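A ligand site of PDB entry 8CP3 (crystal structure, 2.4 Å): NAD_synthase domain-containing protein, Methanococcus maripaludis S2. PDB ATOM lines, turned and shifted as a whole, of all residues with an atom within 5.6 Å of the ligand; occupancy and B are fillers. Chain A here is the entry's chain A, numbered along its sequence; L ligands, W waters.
O12 of the ligand lies within hydrogen-bond range of O of Ala 38 (2.4 Å).
O6 of the ligand lies within salt-bridge range of NH1 of Arg 143 (2.5 Å).
OG of Ser 40 lies within hydrogen-bond range of O1 of the ligand (2.8 Å).
The backbone NH (N) of Ser 45 is in hydrogen-bond range of an oxygen (O1) of the ligand (3.2 Å).
OG of Ser 45 sits at hydrogen-bond distance from O1 of the ligand, 2.9 Å away.
The backbone NH (N) of Ile 63 is in hydrogen-bond range of a nitrogen (N5) of the ligand.
A nitrogen (N4) of the ligand lies within hydrogen-bond range of the backbone carbonyl oxygen (O) of Ile 63, at 2.9 Å.
N of Gly 133 is in hydrogen-bond range of O12 of the ligand.
O7 of the ligand lies within salt-bridge range of NZ of Lys 111, at 3.0 Å.
The backbone NH (N) of Asp 44 sits at hydrogen-bond distance from an oxygen (O3) of the ligand.
N of Gly 42 lies close to O1 of the ligand (3.4 Å).
The backbone NH of Tyr 39 is in hydrogen-bond range of a nitrogen (N6) of the ligand, 3.4 Å away.
The backbone NH (N) of Ala 38 sits at hydrogen-bond distance from the backbone carbonyl oxygen (O) of Val 131 (2.9 Å).
The side-chain carboxylate of Asp 138 is in salt-bridge range of the guanidinium group of Arg 143 (3.3 Å).
The backbone NH (N) of Ser 40 sits at hydrogen-bond distance from the side-chain hydroxyl (OG) of Ser 45 (3.1 Å).
OG of Ser 40 lies close to N of Gly 42 (3.4 Å).
The side-chain carboxylate of Asp 44 lies within salt-bridge range of the side-chain amino group of Lys 165, at 3.4 Å.
The side-chain hydroxyl (OG1) of Thr 46 sits at hydrogen-bond distance from the backbone carbonyl oxygen (O) of Gly 42, 2.8 Å away.
The backbone NH of Tyr 39 is in hydrogen-bond range of the backbone carbonyl oxygen of Val 61 (2.9 Å).
The side-chain carboxylate (OD1) of Asp 132 sits at hydrogen-bond distance from the backbone NH (N) of Thr 134 (3.2 Å).
N of Val 43 touches O3 of the ligand, at 3.6 Å.
Val 61 touches the ligand.
Thr 62 touches the ligand (CA to N5, 3.8 Å).
CE2 of Phe 68 touches N4 of the ligand, 3.2 Å away.
Ile 114 touches the ligand (CD1 to N4, 3.99 Å).
Asp 132 touches the ligand.
Thr 134 touches the ligand (OG1 to C1, 3.5 Å).
Phe 149 touches the ligand (CE2 to O10, 3.5 Å).
Hydrophobic or aromatic side chains within 4 Å of the ligand: Ala 38, Ile 63, Phe 68, Ile 114 and Phe 149.
18 residues have an atom within 4 Å of the ligand: Ala 38, Tyr 39, Ser 40, Gly 42, Val 43, Asp 44, Ser 45, Val 61, Thr 62, Ile 63, Phe 68, Lys 111, Ile 114, Asp 132, Gly 133, Thr 134, Arg 143 and Phe 149.
Water W1 lies within hydrogen-bond range of an oxygen (O6) of the ligand (2.7 Å), the side-chain carboxylate (OD2) of Asp 138 (2.8 Å), the side-chain hydroxyl (OG1) of Thr 134 (2.8 Å) and the guanidinium group (NH1) of Arg 143 (3.4 Å).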
ATOM      1  N   ALA A  38      26.972  30.076  19.576  1.00  0.00           N
ATOM      2  CA  ALA A  38      25.902  29.469  20.359  1.00  0.00           C
ATOM      3  C   ALA A  38      24.899  28.909  19.351  1.00  0.00           C
ATOM      4  O   ALA A  38      24.148  29.657  18.735  1.00  0.00           O
ATOM      5  CB  ALA A  38      25.269  30.540  21.247  1.00  0.00           C
ATOM      6  N   TYR A  39      24.906  27.590  19.167  1.00  0.00           N
ATOM      7  CA  TYR A  39      24.200  26.946  18.042  1.00  0.00           C
ATOM      8  C   TYR A  39      23.091  26.031  18.570  1.00  0.00           C
ATOM      9  O   TYR A  39      23.362  25.096  19.335  1.00  0.00           O
ATOM     10  CB  TYR A  39      25.165  26.128  17.179  1.00  0.00           C
ATOM     11  CG  TYR A  39      24.567  25.278  16.061  1.00  0.00           C
ATOM     12  CD1 TYR A  39      23.866  25.838  14.982  1.00  0.00           C
ATOM     13  CD2 TYR A  39      24.716  23.888  16.071  1.00  0.00           C
ATOM     14  CE1 TYR A  39      23.320  25.016  13.948  1.00  0.00           C
ATOM     15  CE2 TYR A  39      24.186  23.084  15.044  1.00  0.00           C
ATOM     16  CZ  TYR A  39      23.500  23.663  14.010  1.00  0.00           C
ATOM     17  OH  TYR A  39      22.985  22.849  13.031  1.00  0.00           O
ATOM     18  N   SER A  40      21.865  26.288  18.126  1.00  0.00           N
ATOM     19  CA  SER A  40      20.720  25.502  18.566  1.00  0.00           C
ATOM     20  C   SER A  40      20.173  24.587  17.470  1.00  0.00           C
ATOM     21  O   SER A  40      19.269  23.809  17.744  1.00  0.00           O
ATOM     22  CB  SER A  40      19.594  26.421  19.047  1.00  0.00           C
ATOM     23  OG  SER A  40      19.093  27.168  17.938  1.00  0.00           O
ATOM     24  N   GLY A  41      20.692  24.687  16.245  1.00  0.00           N
ATOM     25  CA  GLY A  41      20.139  23.960  15.119  1.00  0.00           C
ATOM     26  C   GLY A  41      19.054  24.686  14.383  1.00  0.00           C
ATOM     27  O   GLY A  41      18.678  24.261  13.274  1.00  0.00           O
ATOM     28  N   GLY A  42      18.504  25.762  14.949  1.00  0.00           N
ATOM     29  CA  GLY A  42      17.458  26.475  14.246  1.00  0.00           C
ATOM     30  C   GLY A  42      18.050  27.252  13.085  1.00  0.00           C
ATOM     31  O   GLY A  42      19.262  27.412  12.955  1.00  0.00           O
ATOM     32  N   VAL A  43      17.143  27.750  12.245  1.00  0.00           N
ATOM     33  CA  VAL A  43      17.534  28.466  11.039  1.00  0.00           C
ATOM     34  C   VAL A  43      18.492  29.618  11.358  1.00  0.00           C
ATOM     35  O   VAL A  43      19.500  29.804  10.659  1.00  0.00           O
ATOM     36  CB  VAL A  43      16.272  28.972  10.320  1.00  0.00           C
ATOM     37  CG1 VAL A  43      16.634  29.715   9.067  1.00  0.00           C
ATOM     38  CG2 VAL A  43      15.357  27.832  10.000  1.00  0.00           C
ATOM     39  N   ASP A  44      18.211  30.387  12.412  1.00  0.00           N
ATOM     40  CA  ASP A  44      18.959  31.627  12.635  1.00  0.00           C
ATOM     41  C   ASP A  44      20.410  31.340  12.998  1.00  0.00           C
ATOM     42  O   ASP A  44      21.334  31.912  12.386  1.00  0.00           O
ATOM     43  CB  ASP A  44      18.286  32.445  13.736  1.00  0.00           C
ATOM     44  CG  ASP A  44      16.897  32.904  13.344  1.00  0.00           C
ATOM     45  OD1 ASP A  44      16.630  33.005  12.114  1.00  0.00           O
ATOM     46  OD2 ASP A  44      16.059  33.136  14.244  1.00  0.00           O
ATOM     47  N   SER A  45      20.641  30.484  13.995  1.00  0.00           N
ATOM     48  CA  SER A  45      21.993  30.181  14.418  1.00  0.00           C
ATOM     49  C   SER A  45      22.700  29.253  13.436  1.00  0.00           C
ATOM     50  O   SER A  45      23.940  29.248  13.401  1.00  0.00           O
ATOM     51  CB  SER A  45      22.010  29.590  15.834  1.00  0.00           C
ATOM     52  OG  SER A  45      21.398  28.316  15.868  1.00  0.00           O
ATOM     53  N   THR A  46      21.961  28.483  12.639  1.00  0.00           N
ATOM     54  CA  THR A  46      22.625  27.786  11.528  1.00  0.00           C
ATOM     55  C   THR A  46      23.184  28.801  10.540  1.00  0.00           C
ATOM     56  O   THR A  46      24.318  28.659  10.072  1.00  0.00           O
ATOM     57  CB  THR A  46      21.689  26.818  10.780  1.00  0.00           C
ATOM     58  OG1 THR A  46      21.156  25.831  11.685  1.00  0.00           O
ATOM     59  CG2 THR A  46      22.441  26.092   9.689  1.00  0.00           C
ATOM     60  N   VAL A  61      28.664  25.602  19.305  1.00  0.00           N
ATOM     61  CA  VAL A  61      28.526  24.916  20.587  1.00  0.00           C
ATOM     62  C   VAL A  61      27.038  24.803  20.909  1.00  0.00           C
ATOM     63  O   VAL A  61      26.322  25.816  20.917  1.00  0.00           O
ATOM     64  CB  VAL A  61      29.297  25.666  21.688  1.00  0.00           C
ATOM     65  CG1 VAL A  61      29.133  24.974  23.059  1.00  0.00           C
ATOM     66  CG2 VAL A  61      30.780  25.723  21.305  1.00  0.00           C
ATOM     67  N   THR A  62      26.563  23.573  21.098  1.00  0.00           N
ATOM     68  CA  THR A  62      25.182  23.309  21.504  1.00  0.00           C
ATOM     69  C   THR A  62      25.217  22.862  22.961  1.00  0.00           C
ATOM     70  O   THR A  62      25.912  21.889  23.282  1.00  0.00           O
ATOM     71  CB  THR A  62      24.528  22.240  20.632  1.00  0.00           C
ATOM     72  OG1 THR A  62      24.624  22.614  19.242  1.00  0.00           O
ATOM     73  CG2 THR A  62      23.043  22.063  20.995  1.00  0.00           C
ATOM     74  N   ILE A  63      24.508  23.580  23.837  1.00  0.00           N
ATOM     75  CA  ILE A  63      24.426  23.215  25.246  1.00  0.00           C
ATOM     76  C   ILE A  63      23.211  22.336  25.461  1.00  0.00           C
ATOM     77  O   ILE A  63      22.075  22.779  25.279  1.00  0.00           O
ATOM     78  CB  ILE A  63      24.392  24.463  26.149  1.00  0.00           C
ATOM     79  CG1 ILE A  63      25.638  25.326  25.945  1.00  0.00           C
ATOM     80  CG2 ILE A  63      24.299  24.051  27.600  1.00  0.00           C
ATOM     81  CD1 ILE A  63      26.938  24.568  26.044  1.00  0.00           C
ATOM     82  N   ASP A  64      23.456  21.120  25.922  1.00  0.00           N
ATOM     83  CA  ASP A  64      22.401  20.170  26.246  1.00  0.00           C
ATOM     84  C   ASP A  64      22.075  20.269  27.744  1.00  0.00           C
ATOM     85  O   ASP A  64      22.772  19.698  28.590  1.00  0.00           O
ATOM     86  CB  ASP A  64      22.871  18.788  25.855  1.00  0.00           C
ATOM     87  CG  ASP A  64      21.929  17.704  26.241  1.00  0.00           C
ATOM     88  OD1 ASP A  64      20.762  17.964  26.640  1.00  0.00           O
ATOM     89  OD2 ASP A  64      22.397  16.557  26.160  1.00  0.00           O
ATOM     90  N   ASN A  65      21.045  21.049  28.075  1.00  0.00           N
ATOM     91  CA  ASN A  65      20.650  21.287  29.460  1.00  0.00           C
ATOM     92  C   ASN A  65      19.417  20.500  29.884  1.00  0.00           C
ATOM     93  O   ASN A  65      18.877  20.784  30.948  1.00  0.00           O
ATOM     94  CB  ASN A  65      20.387  22.770  29.696  1.00  0.00           C
ATOM     95  CG  ASN A  65      19.290  23.317  28.796  1.00  0.00           C
ATOM     96  OD1 ASN A  65      18.730  22.579  27.966  1.00  0.00           O
ATOM     97  ND2 ASN A  65      18.983  24.586  28.953  1.00  0.00           N
ATOM     98  N   PHE A  68      16.075  20.257  25.513  1.00  0.00           N
ATOM     99  CA  PHE A  68      16.023  19.861  24.118  1.00  0.00           C
ATOM    100  C   PHE A  68      16.035  18.348  24.012  1.00  0.00           C
ATOM    101  O   PHE A  68      16.883  17.696  24.628  1.00  0.00           O
ATOM    102  CB  PHE A  68      17.212  20.445  23.374  1.00  0.00           C
ATOM    103  CG  PHE A  68      17.216  21.940  23.317  1.00  0.00           C
ATOM    104  CD1 PHE A  68      16.618  22.599  22.259  1.00  0.00           C
ATOM    105  CD2 PHE A  68      17.784  22.675  24.362  1.00  0.00           C
ATOM    106  CE1 PHE A  68      16.624  23.992  22.198  1.00  0.00           C
ATOM    107  CE2 PHE A  68      17.777  24.067  24.333  1.00  0.00           C
ATOM    108  CZ  PHE A  68      17.204  24.726  23.235  1.00  0.00           C
ATOM    109  N   LYS A 111      18.849  30.593  30.899  1.00  0.00           N
ATOM    110  CA  LYS A 111      19.663  31.031  29.783  1.00  0.00           C
ATOM    111  C   LYS A 111      21.037  31.520  30.250  1.00  0.00           C
ATOM    112  O   LYS A 111      22.022  31.404  29.507  1.00  0.00           O
ATOM    113  CB  LYS A 111      18.922  32.113  29.008  1.00  0.00           C
ATOM    114  CG  LYS A 111      17.613  31.594  28.441  1.00  0.00           C
ATOM    115  CD  LYS A 111      17.510  31.777  26.944  1.00  0.00           C
ATOM    116  CE  LYS A 111      16.398  30.905  26.361  1.00  0.00           C
ATOM    117  NZ  LYS A 111      16.788  30.344  25.000  1.00  0.00           N
ATOM    118  N   ILE A 114      23.342  28.573  30.331  1.00  0.00           N
ATOM    119  CA  ILE A 114      23.885  28.258  29.012  1.00  0.00           C
ATOM    120  C   ILE A 114      24.975  29.258  28.642  1.00  0.00           C
ATOM    121  O   ILE A 114      26.078  28.868  28.224  1.00  0.00           O
ATOM    122  CB  ILE A 114      22.772  28.255  27.947  1.00  0.00           C
ATOM    123  CG1 ILE A 114      21.798  27.091  28.161  1.00  0.00           C
ATOM    124  CG2 ILE A 114      23.381  28.213  26.551  1.00  0.00           C
ATOM    125  CD1 ILE A 114      20.653  27.140  27.191  1.00  0.00           C
ATOM    126  N   LEU A 118      28.949  28.699  27.748  1.00  0.00           N
ATOM    127  CA  LEU A 118      29.556  29.125  26.506  1.00  0.00           C
ATOM    128  C   LEU A 118      30.804  29.945  26.779  1.00  0.00           C
ATOM    129  O   LEU A 118      31.817  29.826  26.066  1.00  0.00           O
ATOM    130  CB  LEU A 118      28.549  29.901  25.660  1.00  0.00           C
ATOM    131  CG  LEU A 118      27.439  29.065  25.024  1.00  0.00           C
ATOM    132  CD1 LEU A 118      26.316  29.934  24.584  1.00  0.00           C
ATOM    133  CD2 LEU A 118      27.997  28.336  23.826  1.00  0.00           C
ATOM    134  N   VAL A 131      29.173  34.447  19.547  1.00  0.00           N
ATOM    135  CA  VAL A 131      28.037  35.046  18.859  1.00  0.00           C
ATOM    136  C   VAL A 131      26.822  34.131  18.966  1.00  0.00           C
ATOM    137  O   VAL A 131      26.935  32.913  19.108  1.00  0.00           O
ATOM    138  CB  VAL A 131      28.351  35.328  17.376  1.00  0.00           C
ATOM    139  CG1 VAL A 131      29.515  36.285  17.300  1.00  0.00           C
ATOM    140  CG2 VAL A 131      28.644  33.980  16.631  1.00  0.00           C
ATOM    141  N   ASP A 132      25.640  34.721  18.843  1.00  0.00           N
ATOM    142  CA  ASP A 132      24.445  33.892  18.875  1.00  0.00           C
ATOM    143  C   ASP A 132      23.574  34.205  17.679  1.00  0.00           C
ATOM    144  O   ASP A 132      23.992  34.960  16.784  1.00  0.00           O
ATOM    145  CB  ASP A 132      23.693  34.060  20.216  1.00  0.00           C
ATOM    146  CG  ASP A 132      23.149  35.471  20.455  1.00  0.00           C
ATOM    147  OD1 ASP A 132      22.834  36.190  19.474  1.00  0.00           O
ATOM    148  OD2 ASP A 132      23.018  35.854  21.647  1.00  0.00           O
ATOM    149  N   GLY A 133      22.375  33.630  17.625  1.00  0.00           N
ATOM    150  CA  GLY A 133      21.527  33.722  16.464  1.00  0.00           C
ATOM    151  C   GLY A 133      20.311  34.589  16.658  1.00  0.00           C
ATOM    152  O   GLY A 133      19.381  34.521  15.835  1.00  0.00           O
ATOM    153  N   THR A 134      20.271  35.411  17.705  1.00  0.00           N
ATOM    154  CA  THR A 134      19.169  36.341  17.904  1.00  0.00           C
ATOM    155  C   THR A 134      19.092  37.325  16.745  1.00  0.00           C
ATOM    156  O   THR A 134      20.096  37.956  16.378  1.00  0.00           O
ATOM    157  CB  THR A 134      19.347  37.092  19.231  1.00  0.00           C
ATOM    158  OG1 THR A 134      19.199  36.185  20.336  1.00  0.00           O
ATOM    159  CG2 THR A 134      18.381  38.266  19.359  1.00  0.00           C
ATOM    160  N   ASP A 138      13.598  39.593  17.063  1.00  0.00           N
ATOM    161  CA  ASP A 138      13.501  38.960  18.383  1.00  0.00           C
ATOM    162  C   ASP A 138      13.528  39.988  19.516  1.00  0.00           C
ATOM    163  O   ASP A 138      12.890  39.787  20.547  1.00  0.00           O
ATOM    164  CB  ASP A 138      14.665  37.993  18.622  1.00  0.00           C
ATOM    165  CG  ASP A 138      14.681  36.797  17.684  1.00  0.00           C
ATOM    166  OD1 ASP A 138      13.670  36.498  17.022  1.00  0.00           O
ATOM    167  OD2 ASP A 138      15.731  36.128  17.627  1.00  0.00           O
ATOM    168  N   ARG A 143      11.573  38.069  25.355  1.00  0.00           N
ATOM    169  CA  ARG A 143      12.310  36.853  25.680  1.00  0.00           C
ATOM    170  C   ARG A 143      13.346  37.134  26.761  1.00  0.00           C
ATOM    171  O   ARG A 143      14.379  37.764  26.461  1.00  0.00           O
ATOM    172  CB  ARG A 143      13.016  36.342  24.422  1.00  0.00           C
ATOM    173  CG  ARG A 143      12.257  36.541  23.134  1.00  0.00           C
ATOM    174  CD  ARG A 143      13.040  35.926  21.980  1.00  0.00           C
ATOM    175  NE  ARG A 143      12.201  35.675  20.805  1.00  0.00           N
ATOM    176  CZ  ARG A 143      12.457  34.745  19.894  1.00  0.00           C
ATOM    177  NH1 ARG A 143      13.436  33.873  20.047  1.00  0.00           N
ATOM    178  NH2 ARG A 143      11.667  34.651  18.827  1.00  0.00           N
ATOM    179  N   PHE A 149      22.293  36.571  27.841  1.00  0.00           N
ATOM    180  CA  PHE A 149      23.419  36.442  26.917  1.00  0.00           C
ATOM    181  C   PHE A 149      24.221  37.742  26.829  1.00  0.00           C
ATOM    182  O   PHE A 149      25.453  37.725  26.784  1.00  0.00           O
ATOM    183  CB  PHE A 149      22.910  36.039  25.534  1.00  0.00           C
ATOM    184  CG  PHE A 149      22.801  34.558  25.333  1.00  0.00           C
ATOM    185  CD1 PHE A 149      22.380  33.721  26.353  1.00  0.00           C
ATOM    186  CD2 PHE A 149      23.082  33.995  24.103  1.00  0.00           C
ATOM    187  CE1 PHE A 149      22.272  32.355  26.158  1.00  0.00           C
ATOM    188  CE2 PHE A 149      22.965  32.618  23.898  1.00  0.00           C
ATOM    189  CZ  PHE A 149      22.570  31.813  24.911  1.00  0.00           C
ATOM    190  N   LYS A 165      13.283  38.384   9.745  1.00  0.00           N
ATOM    191  CA  LYS A 165      13.112  36.965   9.454  1.00  0.00           C
ATOM    192  C   LYS A 165      13.249  36.702   7.959  1.00  0.00           C
ATOM    193  O   LYS A 165      13.876  35.718   7.564  1.00  0.00           O
ATOM    194  CB  LYS A 165      11.756  36.495   9.995  1.00  0.00           C
ATOM    195  CG  LYS A 165      11.378  35.052   9.721  1.00  0.00           C
ATOM    196  CD  LYS A 165      12.411  34.046  10.291  1.00  0.00           C
ATOM    197  CE  LYS A 165      12.402  33.948  11.823  1.00  0.00           C
ATOM    198  NZ  LYS A 165      13.217  32.778  12.331  1.00  0.00           N
HETATM  199  P1  LIG L   1      17.475  29.877  16.283  1.00  0.00           P
HETATM  200  O1  LIG L   1      18.613  28.993  15.901  1.00  0.00           O
HETATM  201  O2  LIG L   1      18.056  31.281  16.635  1.00  0.00           O
HETATM  202  O3  LIG L   1      16.516  29.970  15.022  1.00  0.00           O
HETATM  203  P2  LIG L   1      15.783  30.648  18.471  1.00  0.00           P
HETATM  204  O4  LIG L   1      14.326  30.451  18.236  1.00  0.00           O
HETATM  205  O5  LIG L   1      16.164  32.045  17.899  1.00  0.00           O
HETATM  206  N1  LIG L   1      16.636  29.398  17.685  1.00  0.00           N
HETATM  207  P3  LIG L   1      16.121  31.639  21.203  1.00  0.00           P
HETATM  208  O6  LIG L   1      15.574  32.969  20.871  1.00  0.00           O
HETATM  209  O7  LIG L   1      15.451  30.944  22.375  1.00  0.00           O
HETATM  210  O8  LIG L   1      16.090  30.539  20.015  1.00  0.00           O
HETATM  211  O9  LIG L   1      17.671  31.783  21.522  1.00  0.00           O
HETATM  212  C1  LIG L   1      18.525  32.775  20.935  1.00  0.00           C
HETATM  213  C2  LIG L   1      19.840  32.132  20.543  1.00  0.00           C
HETATM  214  O10 LIG L   1      20.447  31.467  21.679  1.00  0.00           O
HETATM  215  C3  LIG L   1      19.765  31.052  19.488  1.00  0.00           C
HETATM  216  O11 LIG L   1      19.623  31.644  18.202  1.00  0.00           O
HETATM  217  C4  LIG L   1      21.115  30.343  19.677  1.00  0.00           C
HETATM  218  O12 LIG L   1      22.209  31.074  19.133  1.00  0.00           O
HETATM  219  C5  LIG L   1      21.252  30.397  21.206  1.00  0.00           C
HETATM  220  N2  LIG L   1      20.847  29.168  21.864  1.00  0.00           N
HETATM  221  C6  LIG L   1      19.586  28.801  22.250  1.00  0.00           C
HETATM  222  N3  LIG L   1      19.521  27.608  22.808  1.00  0.00           N
HETATM  223  C7  LIG L   1      20.840  27.176  22.788  1.00  0.00           C
HETATM  224  C8  LIG L   1      21.462  25.982  23.243  1.00  0.00           C
HETATM  225  N4  LIG L   1      20.789  24.987  23.833  1.00  0.00           N
HETATM  226  N5  LIG L   1      22.796  25.854  23.053  1.00  0.00           N
HETATM  227  C9  LIG L   1      23.451  26.853  22.463  1.00  0.00           C
HETATM  228  N6  LIG L   1      22.981  28.009  21.997  1.00  0.00           N
HETATM  229  C10 LIG L   1      21.672  28.115  22.202  1.00  0.00           C
HETATM  230  O   HOH W   1      16.511  35.408  20.188  1.00  0.00           O
